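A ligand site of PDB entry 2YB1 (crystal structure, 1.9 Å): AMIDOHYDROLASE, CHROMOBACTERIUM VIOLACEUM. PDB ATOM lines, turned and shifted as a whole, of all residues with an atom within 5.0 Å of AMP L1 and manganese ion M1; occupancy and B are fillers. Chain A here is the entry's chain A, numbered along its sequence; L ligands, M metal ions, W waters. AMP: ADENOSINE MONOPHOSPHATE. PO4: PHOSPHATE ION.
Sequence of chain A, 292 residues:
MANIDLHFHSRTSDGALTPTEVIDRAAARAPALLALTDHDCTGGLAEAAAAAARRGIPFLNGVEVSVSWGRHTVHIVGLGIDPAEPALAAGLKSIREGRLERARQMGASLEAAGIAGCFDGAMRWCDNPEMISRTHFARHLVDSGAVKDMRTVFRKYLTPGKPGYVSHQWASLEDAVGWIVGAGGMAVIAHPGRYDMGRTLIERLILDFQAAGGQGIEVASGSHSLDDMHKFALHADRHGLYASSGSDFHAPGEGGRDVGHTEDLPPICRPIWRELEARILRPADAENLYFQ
The side-chain hydroxyl (OG) of Ser 133 sits at hydrogen-bond distance from an oxygen (O5') of AMP L1 (3.3 Å). An oxygen (O1P) of AMP L1 lies within salt-bridge range of the guanidinium group (NE) of Arg 134, at 2.8 Å. An oxygen (O3P) of AMP L1 lies within hydrogen-bond range of the backbone NH of Arg 134. NH2 of Arg 99 is in salt-bridge range of O2P of AMP L1. An oxygen (O3P) of AMP L1 lies within salt-bridge range of the guanidinium group (NH1) of Arg 102 (2.8 Å). The side-chain hydroxyl of Thr 135 lies within hydrogen-bond range of an oxygen (O4') of AMP L1.
OD1 of Asp 14 sits at hydrogen-bond distance from ND1 of His 9. The side-chain carboxylate (OD2) of Asp 14 sits close to the side-chain hydroxyl (OG1) of Thr 135 (2.7 Å). The backbone carbonyl oxygen (O) of Ile 132 is in hydrogen-bond range of the guanidinium group (NH1) of Arg 99 (3.0 Å). N of Thr 135 is in hydrogen-bond range of OG of Ser 133.
CE1 of His 75 touches O3' of AMP L1, 3.9 Å away. CD2 of Phe 154 touches C6 of AMP L1 (3.4 Å). Hydrophobic or aromatic side chains that line AMP L1: His 39, His 75, Phe 154 and His 250. Ten residues have an atom within 4 Å of AMP L1: Asp 14, His 39, His 75, Arg 99, Arg 102, Ser 133, Arg 134, Thr 135, Phe 154 and His 250. The nearest printed residue that does not touch AMP L1 is Ile 132 (4.4 Å).
CE1 of His 9 touches manganese ion M1, 3.9 Å away. Within 4 Å of manganese ion M1: His 9, Asp 14, His 39 and His 250.
OD2 of Asp 14 is bound to manganese ion M1, 2.2 Å away. O2 of PO4 L2 is bound to manganese ion M1, at 2.2 Å. NE2 of His 39 binds manganese ion M1. A ring nitrogen (NE2) of His 250 is bound to manganese ion M1, at 2.3 Å. Manganese ion M1 is bound by an oxygen (O2') of AMP L1. An oxygen (O3') of AMP L1 is bound to manganese ion M1 (2.5 Å). Slightly farther from manganese ion M1 lies OD1 of Asp 14 (2.9 Å).
Water W1 lies within hydrogen-bond range of O1P of AMP L1 (2.6 Å), NH2 of Arg 134 (3.5 Å) and NE1 of Trp 170 (3.5 Å). Water W3 lies within hydrogen-bond range of an oxygen (O2P) of AMP L1 (2.8 Å), a ring nitrogen (NE2) of His 75 (2.8 Å) and the side-chain hydroxyl of Ser 66 (2.9 Å). Water W4 bridges the side-chain hydroxyl of Ser 133 (2.8 Å) and an oxygen (O2P) of AMP L1 (3.2 Å).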
ATOM      1  N   HIS A   9      -6.866  12.817  -2.172  1.00  0.00           N
ATOM      2  CA  HIS A   9      -6.231  14.124  -2.047  1.00  0.00           C
ATOM      3  C   HIS A   9      -4.808  14.051  -1.522  1.00  0.00           C
ATOM      4  O   HIS A   9      -4.407  13.045  -0.932  1.00  0.00           O
ATOM      5  CB  HIS A   9      -7.053  15.033  -1.125  1.00  0.00           C
ATOM      6  CG  HIS A   9      -8.408  15.329  -1.677  1.00  0.00           C
ATOM      7  ND1 HIS A   9      -8.668  16.467  -2.415  1.00  0.00           N
ATOM      8  CD2 HIS A   9      -9.553  14.621  -1.659  1.00  0.00           C
ATOM      9  CE1 HIS A   9      -9.927  16.446  -2.802  1.00  0.00           C
ATOM     10  NE2 HIS A   9     -10.484  15.344  -2.360  1.00  0.00           N
ATOM     11  N   ASP A  14      -6.094  19.672   0.114  1.00  0.00           N
ATOM     12  CA  ASP A  14      -6.451  19.381   1.510  1.00  0.00           C
ATOM     13  C   ASP A  14      -6.083  18.018   2.115  1.00  0.00           C
ATOM     14  O   ASP A  14      -6.532  17.689   3.212  1.00  0.00           O
ATOM     15  CB  ASP A  14      -7.876  19.840   1.870  1.00  0.00           C
ATOM     16  CG  ASP A  14      -8.922  18.980   1.232  1.00  0.00           C
ATOM     17  OD1 ASP A  14      -8.566  18.151   0.376  1.00  0.00           O
ATOM     18  OD2 ASP A  14     -10.099  19.142   1.602  1.00  0.00           O
ATOM     19  N   HIS A  39      -8.408  19.361  -5.051  1.00  0.00           N
ATOM     20  CA  HIS A  39      -9.372  20.445  -5.260  1.00  0.00           C
ATOM     21  C   HIS A  39      -8.797  21.560  -6.115  1.00  0.00           C
ATOM     22  O   HIS A  39      -7.744  22.107  -5.783  1.00  0.00           O
ATOM     23  CB  HIS A  39      -9.756  21.061  -3.914  1.00  0.00           C
ATOM     24  CG  HIS A  39     -10.526  20.148  -3.011  1.00  0.00           C
ATOM     25  ND1 HIS A  39     -11.845  19.827  -3.243  1.00  0.00           N
ATOM     26  CD2 HIS A  39     -10.176  19.529  -1.869  1.00  0.00           C
ATOM     27  CE1 HIS A  39     -12.275  19.034  -2.270  1.00  0.00           C
ATOM     28  NE2 HIS A  39     -11.283  18.834  -1.426  1.00  0.00           N
ATOM     29  N   SER A  66     -14.627  22.734  -7.744  1.00  0.00           N
ATOM     30  CA  SER A  66     -15.676  23.334  -6.910  1.00  0.00           C
ATOM     31  C   SER A  66     -16.659  24.098  -7.792  1.00  0.00           C
ATOM     32  O   SER A  66     -16.261  24.918  -8.620  1.00  0.00           O
ATOM     33  CB  SER A  66     -15.067  24.313  -5.905  1.00  0.00           C
ATOM     34  OG  SER A  66     -14.037  23.709  -5.126  1.00  0.00           O
ATOM     35  N   HIS A  75     -19.321  19.184  -6.231  1.00  0.00           N
ATOM     36  CA  HIS A  75     -17.962  18.928  -6.682  1.00  0.00           C
ATOM     37  C   HIS A  75     -17.956  18.036  -7.913  1.00  0.00           C
ATOM     38  O   HIS A  75     -18.600  16.981  -7.925  1.00  0.00           O
ATOM     39  CB  HIS A  75     -17.135  18.298  -5.556  1.00  0.00           C
ATOM     40  CG  HIS A  75     -16.784  19.254  -4.463  1.00  0.00           C
ATOM     41  ND1 HIS A  75     -16.267  18.856  -3.249  1.00  0.00           N
ATOM     42  CD2 HIS A  75     -16.866  20.608  -4.400  1.00  0.00           C
ATOM     43  CE1 HIS A  75     -16.038  19.907  -2.491  1.00  0.00           C
ATOM     44  NE2 HIS A  75     -16.383  20.986  -3.175  1.00  0.00           N
ATOM     45  N   ARG A  99      -9.769  32.282  -2.685  1.00  0.00           N
ATOM     46  CA  ARG A  99      -9.647  31.323  -1.590  1.00  0.00           C
ATOM     47  C   ARG A  99      -8.977  31.921  -0.350  1.00  0.00           C
ATOM     48  O   ARG A  99      -9.486  31.794   0.770  1.00  0.00           O
ATOM     49  CB  ARG A  99      -8.914  30.066  -2.073  1.00  0.00           C
ATOM     50  CG  ARG A  99      -9.315  28.787  -1.375  1.00  0.00           C
ATOM     51  CD  ARG A  99      -8.846  27.560  -2.139  1.00  0.00           C
ATOM     52  NE  ARG A  99      -9.961  26.731  -2.630  1.00  0.00           N
ATOM     53  CZ  ARG A  99     -10.850  26.125  -1.845  1.00  0.00           C
ATOM     54  NH1 ARG A  99     -10.789  26.248  -0.521  1.00  0.00           N
ATOM     55  NH2 ARG A  99     -11.834  25.392  -2.387  1.00  0.00           N
ATOM     56  N   ARG A 102     -11.201  34.631   1.316  1.00  0.00           N
ATOM     57  CA  ARG A 102     -12.280  33.965   2.028  1.00  0.00           C
ATOM     58  C   ARG A 102     -11.807  33.381   3.352  1.00  0.00           C
ATOM     59  O   ARG A 102     -12.512  33.423   4.373  1.00  0.00           O
ATOM     60  CB  ARG A 102     -12.852  32.864   1.145  1.00  0.00           C
ATOM     61  CG  ARG A 102     -13.870  31.917   1.793  1.00  0.00           C
ATOM     62  CD  ARG A 102     -14.266  30.879   0.716  1.00  0.00           C
ATOM     63  NE  ARG A 102     -15.187  29.827   1.144  1.00  0.00           N
ATOM     64  CZ  ARG A 102     -14.819  28.577   1.420  1.00  0.00           C
ATOM     65  NH1 ARG A 102     -13.532  28.212   1.336  1.00  0.00           N
ATOM     66  NH2 ARG A 102     -15.743  27.680   1.773  1.00  0.00           N
ATOM     67  N   ILE A 132      -5.872  27.126   0.705  1.00  0.00           N
ATOM     68  CA  ILE A 132      -6.409  27.109   2.064  1.00  0.00           C
ATOM     69  C   ILE A 132      -7.913  26.751   2.091  1.00  0.00           C
ATOM     70  O   ILE A 132      -8.712  27.324   1.340  1.00  0.00           O
ATOM     71  CB  ILE A 132      -6.136  28.470   2.793  1.00  0.00           C
ATOM     72  CG1 ILE A 132      -6.627  28.449   4.242  1.00  0.00           C
ATOM     73  CG2 ILE A 132      -6.760  29.654   2.023  1.00  0.00           C
ATOM     74  CD1 ILE A 132      -5.801  27.568   5.189  1.00  0.00           C
ATOM     75  N   SER A 133      -8.282  25.830   2.963  1.00  0.00           N
ATOM     76  CA  SER A 133      -9.582  25.155   2.881  1.00  0.00           C
ATOM     77  C   SER A 133     -10.238  25.025   4.259  1.00  0.00           C
ATOM     78  O   SER A 133      -9.549  25.051   5.265  1.00  0.00           O
ATOM     79  CB  SER A 133      -9.334  23.759   2.299  1.00  0.00           C
ATOM     80  OG  SER A 133     -10.340  22.829   2.625  1.00  0.00           O
ATOM     81  N   ARG A 134     -11.568  24.894   4.300  1.00  0.00           N
ATOM     82  CA  ARG A 134     -12.277  24.578   5.534  1.00  0.00           C
ATOM     83  C   ARG A 134     -11.665  23.347   6.205  1.00  0.00           C
ATOM     84  O   ARG A 134     -11.746  23.213   7.432  1.00  0.00           O
ATOM     85  CB  ARG A 134     -13.771  24.314   5.287  1.00  0.00           C
ATOM     86  CG  ARG A 134     -14.562  25.568   4.917  1.00  0.00           C
ATOM     87  CD  ARG A 134     -16.068  25.296   4.861  1.00  0.00           C
ATOM     88  NE  ARG A 134     -16.444  24.563   3.654  1.00  0.00           N
ATOM     89  CZ  ARG A 134     -17.539  23.820   3.541  1.00  0.00           C
ATOM     90  NH1 ARG A 134     -18.378  23.699   4.567  1.00  0.00           N
ATOM     91  NH2 ARG A 134     -17.805  23.194   2.397  1.00  0.00           N
ATOM     92  N   THR A 135     -11.088  22.451   5.413  1.00  0.00           N
ATOM     93  CA  THR A 135     -10.467  21.233   5.957  1.00  0.00           C
ATOM     94  C   THR A 135      -9.320  21.585   6.887  1.00  0.00           C
ATOM     95  O   THR A 135      -9.188  21.000   7.957  1.00  0.00           O
ATOM     96  CB  THR A 135      -9.932  20.317   4.834  1.00  0.00           C
ATOM     97  OG1 THR A 135     -11.015  19.947   3.967  1.00  0.00           O
ATOM     98  CG2 THR A 135      -9.291  19.044   5.413  1.00  0.00           C
ATOM     99  N   MET A 150     -13.447  15.985  13.831  1.00  0.00           N
ATOM    100  CA  MET A 150     -13.789  16.612  12.546  1.00  0.00           C
ATOM    101  C   MET A 150     -15.298  16.717  12.362  1.00  0.00           C
ATOM    102  O   MET A 150     -15.804  17.727  11.848  1.00  0.00           O
ATOM    103  CB  MET A 150     -13.184  15.831  11.375  1.00  0.00           C
ATOM    104  CG  MET A 150     -11.659  15.809  11.342  1.00  0.00           C
ATOM    105  SD  MET A 150     -10.908  17.348  10.772  1.00  0.00           S
ATOM    106  CE  MET A 150     -11.177  17.243   8.992  1.00  0.00           C
ATOM    107  N   PHE A 154     -17.861  20.482  11.934  1.00  0.00           N
ATOM    108  CA  PHE A 154     -18.776  20.927  10.891  1.00  0.00           C
ATOM    109  C   PHE A 154     -20.222  20.969  11.356  1.00  0.00           C
ATOM    110  O   PHE A 154     -21.095  21.551  10.710  1.00  0.00           O
ATOM    111  CB  PHE A 154     -18.594  20.061   9.631  1.00  0.00           C
ATOM    112  CG  PHE A 154     -17.289  20.321   8.923  1.00  0.00           C
ATOM    113  CD1 PHE A 154     -17.189  21.342   7.991  1.00  0.00           C
ATOM    114  CD2 PHE A 154     -16.162  19.578   9.231  1.00  0.00           C
ATOM    115  CE1 PHE A 154     -15.976  21.601   7.361  1.00  0.00           C
ATOM    116  CE2 PHE A 154     -14.950  19.837   8.602  1.00  0.00           C
ATOM    117  CZ  PHE A 154     -14.853  20.848   7.661  1.00  0.00           C
ATOM    118  N   TRP A 170     -18.308  29.569  -6.567  1.00  0.00           N
ATOM    119  CA  TRP A 170     -17.290  28.796  -7.276  1.00  0.00           C
ATOM    120  C   TRP A 170     -17.608  28.759  -8.779  1.00  0.00           C
ATOM    121  O   TRP A 170     -18.326  29.621  -9.281  1.00  0.00           O
ATOM    122  CB  TRP A 170     -17.158  27.390  -6.675  1.00  0.00           C
ATOM    123  CG  TRP A 170     -16.999  27.395  -5.190  1.00  0.00           C
ATOM    124  CD1 TRP A 170     -17.966  27.101  -4.265  1.00  0.00           C
ATOM    125  CD2 TRP A 170     -15.819  27.715  -4.446  1.00  0.00           C
ATOM    126  NE1 TRP A 170     -17.443  27.208  -2.991  1.00  0.00           N
ATOM    127  CE2 TRP A 170     -16.135  27.584  -3.080  1.00  0.00           C
ATOM    128  CE3 TRP A 170     -14.520  28.085  -4.806  1.00  0.00           C
ATOM    129  CZ2 TRP A 170     -15.195  27.815  -2.057  1.00  0.00           C
ATOM    130  CZ3 TRP A 170     -13.577  28.322  -3.791  1.00  0.00           C
ATOM    131  CH2 TRP A 170     -13.930  28.175  -2.436  1.00  0.00           C
ATOM    132  N   ARG A 194     -23.826  13.137  -0.557  1.00  0.00           N
ATOM    133  CA  ARG A 194     -23.541  14.201   0.408  1.00  0.00           C
ATOM    134  C   ARG A 194     -24.404  15.444   0.191  1.00  0.00           C
ATOM    135  O   ARG A 194     -24.506  16.294   1.069  1.00  0.00           O
ATOM    136  CB  ARG A 194     -22.063  14.621   0.375  1.00  0.00           C
ATOM    137  CG  ARG A 194     -21.078  13.557   0.807  1.00  0.00           C
ATOM    138  CD  ARG A 194     -20.157  14.083   1.917  1.00  0.00           C
ATOM    139  NE  ARG A 194     -19.594  15.410   1.639  1.00  0.00           N
ATOM    140  CZ  ARG A 194     -18.300  15.647   1.377  1.00  0.00           C
ATOM    141  NH1 ARG A 194     -17.433  14.644   1.340  1.00  0.00           N
ATOM    142  NH2 ARG A 194     -17.886  16.891   1.152  1.00  0.00           N
ATOM    143  N   HIS A 250      -8.293  11.581   2.596  1.00  0.00           N
ATOM    144  CA  HIS A 250      -7.596  12.828   2.956  1.00  0.00           C
ATOM    145  C   HIS A 250      -6.436  12.534   3.889  1.00  0.00           C
ATOM    146  O   HIS A 250      -5.319  12.996   3.673  1.00  0.00           O
ATOM    147  CB  HIS A 250      -8.523  13.854   3.628  1.00  0.00           C
ATOM    148  CG  HIS A 250      -9.462  14.531   2.693  1.00  0.00           C
ATOM    149  ND1 HIS A 250     -10.515  13.875   2.087  1.00  0.00           N
ATOM    150  CD2 HIS A 250      -9.524  15.813   2.262  1.00  0.00           C
ATOM    151  CE1 HIS A 250     -11.187  14.720   1.326  1.00  0.00           C
ATOM    152  NE2 HIS A 250     -10.601  15.905   1.415  1.00  0.00           N
HETATM  153  P   AMP L   1     -13.651  24.480   1.027  1.00  0.00           P
HETATM  154  O1P AMP L   1     -15.089  24.899   1.242  1.00  0.00           O
HETATM  155  O2P AMP L   1     -13.503  24.050  -0.422  1.00  0.00           O
HETATM  156  O3P AMP L   1     -12.720  25.551   1.548  1.00  0.00           O
HETATM  157  O5' AMP L   1     -13.564  23.201   1.972  1.00  0.00           O
HETATM  158  C5' AMP L   1     -14.336  22.046   1.695  1.00  0.00           C
HETATM  159  C4' AMP L   1     -13.672  20.797   2.223  1.00  0.00           C
HETATM  160  O4' AMP L   1     -13.948  20.678   3.638  1.00  0.00           O
HETATM  161  C3' AMP L   1     -14.181  19.490   1.629  1.00  0.00           C
HETATM  162  O3' AMP L   1     -13.569  19.174   0.392  1.00  0.00           O
HETATM  163  C2' AMP L   1     -13.889  18.463   2.731  1.00  0.00           C
HETATM  164  O2' AMP L   1     -12.538  18.033   2.652  1.00  0.00           O
HETATM  165  C1' AMP L   1     -14.057  19.310   3.997  1.00  0.00           C
HETATM  166  N9  AMP L   1     -15.376  19.090   4.625  1.00  0.00           N
HETATM  167  C8  AMP L   1     -16.523  19.735   4.319  1.00  0.00           C
HETATM  168  N7  AMP L   1     -17.550  19.271   5.084  1.00  0.00           N
HETATM  169  C5  AMP L   1     -17.049  18.309   5.892  1.00  0.00           C
HETATM  170  C6  AMP L   1     -17.569  17.415   6.952  1.00  0.00           C
HETATM  171  N6  AMP L   1     -18.879  17.446   7.310  1.00  0.00           N
HETATM  172  N1  AMP L   1     -16.709  16.562   7.552  1.00  0.00           N
HETATM  173  C2  AMP L   1     -15.400  16.512   7.207  1.00  0.00           C
HETATM  174  N3  AMP L   1     -14.853  17.297   6.260  1.00  0.00           N
HETATM  175  C4  AMP L   1     -15.616  18.198   5.590  1.00  0.00           C
HETATM  176  P   PO4 L   2     -14.306  16.184  -0.574  1.00  0.00           P
HETATM  177  O1  PO4 L   2     -14.743  15.468   0.685  1.00  0.00           O
HETATM  178  O2  PO4 L   2     -12.834  16.452  -0.496  1.00  0.00           O
HETATM  179  O3  PO4 L   2     -14.552  15.320  -1.793  1.00  0.00           O
HETATM  180  O4  PO4 L   2     -15.091  17.466  -0.698  1.00  0.00           O
HETATM  181 MN    MN M   1     -11.460  17.824   0.528  1.00  0.00          MN
HETATM  182 MN    MN M   2     -12.607  15.010  -2.575  1.00  0.00          MN
HETATM  183 MN    MN M   3     -15.794  16.728  -2.785  1.00  0.00          MN
HETATM  184  O   HOH W   1     -16.976  24.708  -0.600  1.00  0.00           O
HETATM  185  O   HOH W   2     -12.527  16.392   4.624  1.00  0.00           O
HETATM  186  O   HOH W   3     -15.235  23.410  -2.467  1.00  0.00           O
HETATM  187  O   HOH W   4     -10.855  22.264  -0.045  1.00  0.00           O
